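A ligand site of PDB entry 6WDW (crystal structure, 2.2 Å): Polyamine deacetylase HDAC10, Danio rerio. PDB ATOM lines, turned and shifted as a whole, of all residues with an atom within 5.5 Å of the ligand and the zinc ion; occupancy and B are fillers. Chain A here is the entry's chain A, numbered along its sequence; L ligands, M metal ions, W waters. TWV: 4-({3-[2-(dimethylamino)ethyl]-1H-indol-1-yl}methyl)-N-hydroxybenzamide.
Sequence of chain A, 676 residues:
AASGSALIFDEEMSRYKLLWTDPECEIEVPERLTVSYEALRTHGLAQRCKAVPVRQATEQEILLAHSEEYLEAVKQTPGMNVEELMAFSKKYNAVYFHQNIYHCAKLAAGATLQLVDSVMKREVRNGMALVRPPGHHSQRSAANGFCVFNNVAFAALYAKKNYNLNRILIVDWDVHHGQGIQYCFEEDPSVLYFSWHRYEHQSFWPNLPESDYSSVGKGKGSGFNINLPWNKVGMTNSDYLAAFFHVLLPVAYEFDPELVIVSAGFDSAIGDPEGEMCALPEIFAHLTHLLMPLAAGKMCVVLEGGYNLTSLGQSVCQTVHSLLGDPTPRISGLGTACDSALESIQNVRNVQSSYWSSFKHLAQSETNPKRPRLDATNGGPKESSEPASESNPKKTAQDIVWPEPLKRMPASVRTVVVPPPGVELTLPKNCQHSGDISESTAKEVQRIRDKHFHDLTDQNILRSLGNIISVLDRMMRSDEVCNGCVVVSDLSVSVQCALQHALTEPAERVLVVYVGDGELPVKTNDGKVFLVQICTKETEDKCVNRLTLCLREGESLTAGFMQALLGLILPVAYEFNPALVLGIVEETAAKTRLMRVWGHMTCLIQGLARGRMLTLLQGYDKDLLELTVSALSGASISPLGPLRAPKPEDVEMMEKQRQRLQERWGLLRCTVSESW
Water W3 bridges OE1 of Glu 274 (2.6 Å) and NE2 of His 176 (3.0 Å).
The backbone carbonyl oxygen (O) of Ala 94 sits at hydrogen-bond distance from the backbone NH (N) of Phe 146. NE2 of His 136 sits at hydrogen-bond distance from NE2 of His 137. The side-chain carboxylate of Glu 304 sits at hydrogen-bond distance from the backbone NH of His 136. The side-chain carboxylate (OD1) of Asp 267 is in hydrogen-bond range of the backbone NH (N) of Val 175, at 2.8 Å. OD1 of Asp 174 lies within hydrogen-bond range of N of Gly 305 (3.0 Å). O of Ala 94 lies close to N of Gly 145, 3.1 Å away.
Merely in contact with the ligand: Glu 24 (3.2 Å), Trp 205 (3.5 Å), Phe 146 (3.6 Å), Ala 94 (3.7 Å), Pro 273 (3.8 Å), Gly 145 (3.8 Å) and Ile 27 (3.9 Å). Hydrophobic or aromatic side chains that line the ligand: Ile 27, Ala 94, His 136, His 137, Phe 146, His 176, Trp 205 and Tyr 307. 14 residues have an atom within 4 Å of the ligand: Glu 24, Ile 27, Ala 94, His 136, His 137, Gly 145, Phe 146, Asp 174, His 176, Trp 205, Asp 267, Pro 273, Glu 274 and Tyr 307. The nearest printed residue that does not touch the ligand is Gly 305 (4.2 Å).
The side-chain carboxylate (OE2) of Glu 274 lies within salt-bridge range of a nitrogen (N14) of the ligand (2.7 Å). A ring nitrogen (NE2) of His 136 sits close to an oxygen (O01) of the ligand, at 2.7 Å. A ring nitrogen (NE2) of His 137 sits at hydrogen-bond distance from a nitrogen (N02) of the ligand (2.8 Å). OH of Tyr 307 sits close to O25 of the ligand (2.6 Å).
Three residues have an atom within 4 Å of the zinc ion: Asp 174, His 176 and Asp 267. Along chain A the residues within 4 Å of the zinc ion span positions 174 to 267. The nearest printed residue that does not touch the zinc ion is Val 175 (4.2 Å).
The zinc ion is bound by the side-chain carboxylate (OD2) of Asp 174 (2.0 Å), the side-chain carboxylate (OD2) of Asp 267 (2.1 Å), an oxygen (O25) of the ligand (2.2 Å), an oxygen (O01) of the ligand (2.2 Å) and a ring nitrogen (ND1) of His 176 (2.2 Å). Slightly farther from the zinc ion lies OD1 of Asp 174 (2.7 Å).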
ATOM      1  N   PRO A  23     -27.698   7.193  39.558  1.00  0.00           N
ATOM      2  CA  PRO A  23     -27.388   8.165  38.503  1.00  0.00           C
ATOM      3  C   PRO A  23     -26.740   7.518  37.295  1.00  0.00           C
ATOM      4  O   PRO A  23     -26.856   8.069  36.183  1.00  0.00           O
ATOM      5  CB  PRO A  23     -26.435   9.150  39.185  1.00  0.00           C
ATOM      6  CG  PRO A  23     -26.476   8.800  40.668  1.00  0.00           C
ATOM      7  CD  PRO A  23     -26.830   7.351  40.738  1.00  0.00           C
ATOM      8  N   GLU A  24     -26.076   6.378  37.454  1.00  0.00           N
ATOM      9  CA  GLU A  24     -25.498   5.682  36.311  1.00  0.00           C
ATOM     10  C   GLU A  24     -26.576   5.094  35.404  1.00  0.00           C
ATOM     11  O   GLU A  24     -26.431   5.083  34.168  1.00  0.00           O
ATOM     12  CB  GLU A  24     -24.566   4.562  36.788  1.00  0.00           C
ATOM     13  CG  GLU A  24     -23.318   5.032  37.488  1.00  0.00           C
ATOM     14  CD  GLU A  24     -22.240   3.984  37.488  1.00  0.00           C
ATOM     15  OE1 GLU A  24     -22.518   2.855  36.997  1.00  0.00           O
ATOM     16  OE2 GLU A  24     -21.120   4.278  37.949  1.00  0.00           O
ATOM     17  N   CYS A  25     -27.651   4.585  36.006  1.00  0.00           N
ATOM     18  CA  CYS A  25     -28.627   3.784  35.284  1.00  0.00           C
ATOM     19  C   CYS A  25     -29.788   4.591  34.741  1.00  0.00           C
ATOM     20  O   CYS A  25     -30.425   4.176  33.777  1.00  0.00           O
ATOM     21  CB  CYS A  25     -29.182   2.695  36.215  1.00  0.00           C
ATOM     22  SG  CYS A  25     -28.095   1.249  36.323  1.00  0.00           S
ATOM     23  N   ILE A  27     -30.207   6.884  32.853  1.00  0.00           N
ATOM     24  CA  ILE A  27     -30.220   7.336  31.474  1.00  0.00           C
ATOM     25  C   ILE A  27     -30.953   6.362  30.566  1.00  0.00           C
ATOM     26  O   ILE A  27     -31.338   6.729  29.459  1.00  0.00           O
ATOM     27  CB  ILE A  27     -28.796   7.548  30.926  1.00  0.00           C
ATOM     28  CG1 ILE A  27     -28.110   6.181  30.763  1.00  0.00           C
ATOM     29  CG2 ILE A  27     -28.012   8.465  31.851  1.00  0.00           C
ATOM     30  CD1 ILE A  27     -26.614   6.259  30.521  1.00  0.00           C
ATOM     31  N   ALA A  94     -23.426  -1.711  36.643  1.00  0.00           N
ATOM     32  CA  ALA A  94     -24.193  -0.769  35.815  1.00  0.00           C
ATOM     33  C   ALA A  94     -25.378  -1.451  35.120  1.00  0.00           C
ATOM     34  O   ALA A  94     -25.565  -1.387  33.904  1.00  0.00           O
ATOM     35  CB  ALA A  94     -23.278  -0.099  34.801  1.00  0.00           C
ATOM     36  N   HIS A 136     -24.984  -5.850  24.074  1.00  0.00           N
ATOM     37  CA  HIS A 136     -23.606  -6.188  23.716  1.00  0.00           C
ATOM     38  C   HIS A 136     -22.640  -6.205  24.904  1.00  0.00           C
ATOM     39  O   HIS A 136     -21.522  -6.689  24.719  1.00  0.00           O
ATOM     40  CB  HIS A 136     -23.044  -5.247  22.604  1.00  0.00           C
ATOM     41  CG  HIS A 136     -22.826  -3.824  23.030  1.00  0.00           C
ATOM     42  ND1 HIS A 136     -21.975  -2.977  22.356  1.00  0.00           N
ATOM     43  CD2 HIS A 136     -23.353  -3.106  24.046  1.00  0.00           C
ATOM     44  CE1 HIS A 136     -21.992  -1.785  22.924  1.00  0.00           C
ATOM     45  NE2 HIS A 136     -22.825  -1.839  23.962  1.00  0.00           N
ATOM     46  N   HIS A 137     -23.034  -5.744  26.084  1.00  0.00           N
ATOM     47  CA  HIS A 137     -22.206  -5.902  27.280  1.00  0.00           C
ATOM     48  C   HIS A 137     -22.433  -7.213  28.011  1.00  0.00           C
ATOM     49  O   HIS A 137     -21.590  -7.581  28.853  1.00  0.00           O
ATOM     50  CB  HIS A 137     -22.451  -4.781  28.292  1.00  0.00           C
ATOM     51  CG  HIS A 137     -22.069  -3.430  27.800  1.00  0.00           C
ATOM     52  ND1 HIS A 137     -20.874  -3.178  27.161  1.00  0.00           N
ATOM     53  CD2 HIS A 137     -22.743  -2.250  27.814  1.00  0.00           C
ATOM     54  CE1 HIS A 137     -20.816  -1.902  26.810  1.00  0.00           C
ATOM     55  NE2 HIS A 137     -21.941  -1.319  27.193  1.00  0.00           N
ATOM     56  N   GLY A 145     -23.942  -3.409  32.187  1.00  0.00           N
ATOM     57  CA  GLY A 145     -24.169  -2.226  31.372  1.00  0.00           C
ATOM     58  C   GLY A 145     -25.517  -2.191  30.678  1.00  0.00           C
ATOM     59  O   GLY A 145     -25.583  -2.130  29.447  1.00  0.00           O
ATOM     60  N   PHE A 146     -26.600  -2.263  31.463  1.00  0.00           N
ATOM     61  CA  PHE A 146     -28.004  -2.304  31.049  1.00  0.00           C
ATOM     62  C   PHE A 146     -28.364  -3.563  30.275  1.00  0.00           C
ATOM     63  O   PHE A 146     -29.535  -3.751  29.964  1.00  0.00           O
ATOM     64  CB  PHE A 146     -28.432  -1.078  30.205  1.00  0.00           C
ATOM     65  CG  PHE A 146     -27.937   0.233  30.734  1.00  0.00           C
ATOM     66  CD1 PHE A 146     -27.960   0.498  32.083  1.00  0.00           C
ATOM     67  CD2 PHE A 146     -27.436   1.211  29.875  1.00  0.00           C
ATOM     68  CE1 PHE A 146     -27.474   1.709  32.577  1.00  0.00           C
ATOM     69  CE2 PHE A 146     -26.977   2.400  30.354  1.00  0.00           C
ATOM     70  CZ  PHE A 146     -26.987   2.652  31.718  1.00  0.00           C
ATOM     71  N   ASP A 174     -21.693   1.266  18.422  1.00  0.00           N
ATOM     72  CA  ASP A 174     -21.988   1.884  19.707  1.00  0.00           C
ATOM     73  C   ASP A 174     -20.718   2.542  20.230  1.00  0.00           C
ATOM     74  O   ASP A 174     -19.594   2.217  19.818  1.00  0.00           O
ATOM     75  CB  ASP A 174     -22.498   0.811  20.684  1.00  0.00           C
ATOM     76  CG  ASP A 174     -23.035   1.378  21.984  1.00  0.00           C
ATOM     77  OD1 ASP A 174     -24.266   1.452  22.144  1.00  0.00           O
ATOM     78  OD2 ASP A 174     -22.235   1.730  22.882  1.00  0.00           O
ATOM     79  N   VAL A 175     -20.885   3.513  21.133  1.00  0.00           N
ATOM     80  CA  VAL A 175     -19.713   4.244  21.611  1.00  0.00           C
ATOM     81  C   VAL A 175     -19.005   3.517  22.745  1.00  0.00           C
ATOM     82  O   VAL A 175     -17.904   3.935  23.163  1.00  0.00           O
ATOM     83  CB  VAL A 175     -20.079   5.671  22.077  1.00  0.00           C
ATOM     84  CG1 VAL A 175     -20.560   5.664  23.535  1.00  0.00           C
ATOM     85  CG2 VAL A 175     -18.885   6.613  21.846  1.00  0.00           C
ATOM     86  N   HIS A 176     -19.606   2.463  23.273  1.00  0.00           N
ATOM     87  CA  HIS A 176     -19.040   1.629  24.311  1.00  0.00           C
ATOM     88  C   HIS A 176     -18.540   0.321  23.719  1.00  0.00           C
ATOM     89  O   HIS A 176     -19.037  -0.103  22.664  1.00  0.00           O
ATOM     90  CB  HIS A 176     -20.075   1.342  25.385  1.00  0.00           C
ATOM     91  CG  HIS A 176     -20.532   2.553  26.128  1.00  0.00           C
ATOM     92  ND1 HIS A 176     -21.679   3.238  25.795  1.00  0.00           N
ATOM     93  CD2 HIS A 176     -20.016   3.189  27.210  1.00  0.00           C
ATOM     94  CE1 HIS A 176     -21.859   4.234  26.641  1.00  0.00           C
ATOM     95  NE2 HIS A 176     -20.856   4.232  27.505  1.00  0.00           N
ATOM     96  N   TRP A 205     -15.446   3.787  31.019  1.00  0.00           N
ATOM     97  CA  TRP A 205     -16.142   2.534  31.285  1.00  0.00           C
ATOM     98  C   TRP A 205     -16.296   1.748  29.985  1.00  0.00           C
ATOM     99  O   TRP A 205     -16.589   2.337  28.936  1.00  0.00           O
ATOM    100  CB  TRP A 205     -17.491   2.837  31.943  1.00  0.00           C
ATOM    101  CG  TRP A 205     -18.222   1.605  32.413  1.00  0.00           C
ATOM    102  CD1 TRP A 205     -18.255   1.100  33.682  1.00  0.00           C
ATOM    103  CD2 TRP A 205     -18.999   0.731  31.606  1.00  0.00           C
ATOM    104  NE1 TRP A 205     -18.998  -0.062  33.706  1.00  0.00           N
ATOM    105  CE2 TRP A 205     -19.470  -0.313  32.445  1.00  0.00           C
ATOM    106  CE3 TRP A 205     -19.330   0.695  30.245  1.00  0.00           C
ATOM    107  CZ2 TRP A 205     -20.269  -1.369  31.969  1.00  0.00           C
ATOM    108  CZ3 TRP A 205     -20.117  -0.349  29.769  1.00  0.00           C
ATOM    109  CH2 TRP A 205     -20.578  -1.365  30.637  1.00  0.00           C
ATOM    110  N   ASP A 267     -25.256   6.189  20.792  1.00  0.00           N
ATOM    111  CA  ASP A 267     -24.563   7.072  21.706  1.00  0.00           C
ATOM    112  C   ASP A 267     -23.227   7.570  21.143  1.00  0.00           C
ATOM    113  O   ASP A 267     -22.547   8.335  21.829  1.00  0.00           O
ATOM    114  CB  ASP A 267     -24.340   6.398  23.059  1.00  0.00           C
ATOM    115  CG  ASP A 267     -23.886   4.961  22.955  1.00  0.00           C
ATOM    116  OD1 ASP A 267     -23.410   4.495  21.882  1.00  0.00           O
ATOM    117  OD2 ASP A 267     -23.999   4.282  24.003  1.00  0.00           O
ATOM    118  N   PRO A 273     -25.013  12.422  25.757  1.00  0.00           N
ATOM    119  CA  PRO A 273     -24.289  12.771  26.984  1.00  0.00           C
ATOM    120  C   PRO A 273     -23.260  11.738  27.402  1.00  0.00           C
ATOM    121  O   PRO A 273     -22.407  12.049  28.244  1.00  0.00           O
ATOM    122  CB  PRO A 273     -25.405  12.908  28.020  1.00  0.00           C
ATOM    123  CG  PRO A 273     -26.476  11.960  27.537  1.00  0.00           C
ATOM    124  CD  PRO A 273     -26.425  12.087  26.023  1.00  0.00           C
ATOM    125  N   GLU A 274     -23.301  10.521  26.857  1.00  0.00           N
ATOM    126  CA  GLU A 274     -22.359   9.470  27.230  1.00  0.00           C
ATOM    127  C   GLU A 274     -21.192   9.312  26.274  1.00  0.00           C
ATOM    128  O   GLU A 274     -20.048   9.111  26.711  1.00  0.00           O
ATOM    129  CB  GLU A 274     -23.107   8.145  27.374  1.00  0.00           C
ATOM    130  CG  GLU A 274     -24.339   8.299  28.248  1.00  0.00           C
ATOM    131  CD  GLU A 274     -23.960   8.428  29.707  1.00  0.00           C
ATOM    132  OE1 GLU A 274     -23.050   7.668  30.152  1.00  0.00           O
ATOM    133  OE2 GLU A 274     -24.538   9.309  30.405  1.00  0.00           O
ATOM    134  N   GLU A 276     -20.226  11.724  23.880  1.00  0.00           N
ATOM    135  CA  GLU A 276     -19.576  13.036  23.765  1.00  0.00           C
ATOM    136  C   GLU A 276     -18.741  13.142  22.491  1.00  0.00           C
ATOM    137  O   GLU A 276     -17.750  13.883  22.433  1.00  0.00           O
ATOM    138  CB  GLU A 276     -18.720  13.337  24.998  1.00  0.00           C
ATOM    139  CG  GLU A 276     -19.526  13.442  26.297  1.00  0.00           C
ATOM    140  CD  GLU A 276     -18.632  13.588  27.535  1.00  0.00           C
ATOM    141  OE1 GLU A 276     -17.757  14.487  27.522  1.00  0.00           O
ATOM    142  OE2 GLU A 276     -18.781  12.803  28.500  1.00  0.00           O
ATOM    143  N   GLU A 304     -28.593  -0.879  20.090  1.00  0.00           N
ATOM    144  CA  GLU A 304     -27.907  -1.001  21.362  1.00  0.00           C
ATOM    145  C   GLU A 304     -28.225   0.248  22.180  1.00  0.00           C
ATOM    146  O   GLU A 304     -29.328   0.351  22.749  1.00  0.00           O
ATOM    147  CB  GLU A 304     -26.402  -1.263  21.170  1.00  0.00           C
ATOM    148  CG  GLU A 304     -26.099  -2.557  20.395  1.00  0.00           C
ATOM    149  CD  GLU A 304     -26.108  -3.820  21.253  1.00  0.00           C
ATOM    150  OE1 GLU A 304     -26.362  -3.728  22.479  1.00  0.00           O
ATOM    151  OE2 GLU A 304     -25.858  -4.924  20.699  1.00  0.00           O
ATOM    152  N   GLY A 305     -27.301   1.231  22.271  1.00  0.00           N
ATOM    153  CA  GLY A 305     -27.500   2.398  23.095  1.00  0.00           C
ATOM    154  C   GLY A 305     -27.892   3.642  22.301  1.00  0.00           C
ATOM    155  O   GLY A 305     -28.079   3.603  21.086  1.00  0.00           O
ATOM    156  N   GLY A 306     -28.002   4.753  23.019  1.00  0.00           N
ATOM    157  CA  GLY A 306     -28.360   6.041  22.442  1.00  0.00           C
ATOM    158  C   GLY A 306     -29.296   6.780  23.369  1.00  0.00           C
ATOM    159  O   GLY A 306     -30.416   6.318  23.609  1.00  0.00           O
ATOM    160  N   TYR A 307     -28.860   7.914  23.936  1.00  0.00           N
ATOM    161  CA  TYR A 307     -29.497   8.464  25.111  1.00  0.00           C
ATOM    162  C   TYR A 307     -29.990   9.888  24.971  1.00  0.00           C
ATOM    163  O   TYR A 307     -30.781  10.316  25.824  1.00  0.00           O
ATOM    164  CB  TYR A 307     -28.543   8.386  26.314  1.00  0.00           C
ATOM    165  CG  TYR A 307     -28.122   6.987  26.525  1.00  0.00           C
ATOM    166  CD1 TYR A 307     -29.003   6.064  27.048  1.00  0.00           C
ATOM    167  CD2 TYR A 307     -26.859   6.553  26.130  1.00  0.00           C
ATOM    168  CE1 TYR A 307     -28.649   4.757  27.204  1.00  0.00           C
ATOM    169  CE2 TYR A 307     -26.486   5.235  26.286  1.00  0.00           C
ATOM    170  CZ  TYR A 307     -27.391   4.342  26.823  1.00  0.00           C
ATOM    171  OH  TYR A 307     -27.072   3.018  27.013  1.00  0.00           O
HETATM  172  C10 TWV L   1     -23.464   5.424  33.079  1.00  0.00           C
HETATM  173  C13 TWV L   1     -22.348   8.878  33.031  1.00  0.00           C
HETATM  174  C15 TWV L   1     -22.109  11.083  31.887  1.00  0.00           C
HETATM  175  C17 TWV L   1     -21.570   5.930  34.213  1.00  0.00           C
HETATM  176  C20 TWV L   1     -19.390   4.263  34.993  1.00  0.00           C
HETATM  177  C21 TWV L   1     -19.403   5.640  35.318  1.00  0.00           C
HETATM  178  C22 TWV L   1     -20.470   6.436  34.931  1.00  0.00           C
HETATM  179  C24 TWV L   1     -23.749   1.178  29.300  1.00  0.00           C
HETATM  180  C03 TWV L   1     -24.188   1.929  26.880  1.00  0.00           C
HETATM  181  C04 TWV L   1     -23.973   2.174  28.376  1.00  0.00           C
HETATM  182  C05 TWV L   1     -23.891   3.506  28.877  1.00  0.00           C
HETATM  183  C06 TWV L   1     -23.638   3.762  30.246  1.00  0.00           C
HETATM  184  C07 TWV L   1     -23.426   2.713  31.180  1.00  0.00           C
HETATM  185  C08 TWV L   1     -23.170   2.887  32.668  1.00  0.00           C
HETATM  186  C11 TWV L   1     -22.818   6.475  33.683  1.00  0.00           C
HETATM  187  C12 TWV L   1     -23.291   7.899  33.765  1.00  0.00           C
HETATM  188  C16 TWV L   1     -23.766  10.814  33.680  1.00  0.00           C
HETATM  189  C18 TWV L   1     -21.536   4.515  33.902  1.00  0.00           C
HETATM  190  C19 TWV L   1     -20.458   3.701  34.297  1.00  0.00           C
HETATM  191  C23 TWV L   1     -23.502   1.433  30.648  1.00  0.00           C
HETATM  192  N02 TWV L   1     -23.725   0.635  26.376  1.00  0.00           N
HETATM  193  N09 TWV L   1     -22.731   4.206  33.175  1.00  0.00           N
HETATM  194  N14 TWV L   1     -23.077  10.109  32.529  1.00  0.00           N
HETATM  195  O01 TWV L   1     -23.862   0.403  25.039  1.00  0.00           O
HETATM  196  O25 TWV L   1     -24.597   2.741  26.114  1.00  0.00           O
HETATM  197 ZN    ZN M   1     -23.236   2.397  24.463  1.00  0.00          ZN
HETATM  198  O   HOH W   1     -19.570   6.704  31.695  1.00  0.00           O
HETATM  199  O   HOH W   2     -20.218   8.969  30.492  1.00  0.00           O
HETATM  200  O   HOH W   3     -21.157   5.959  29.884  1.00  0.00           O
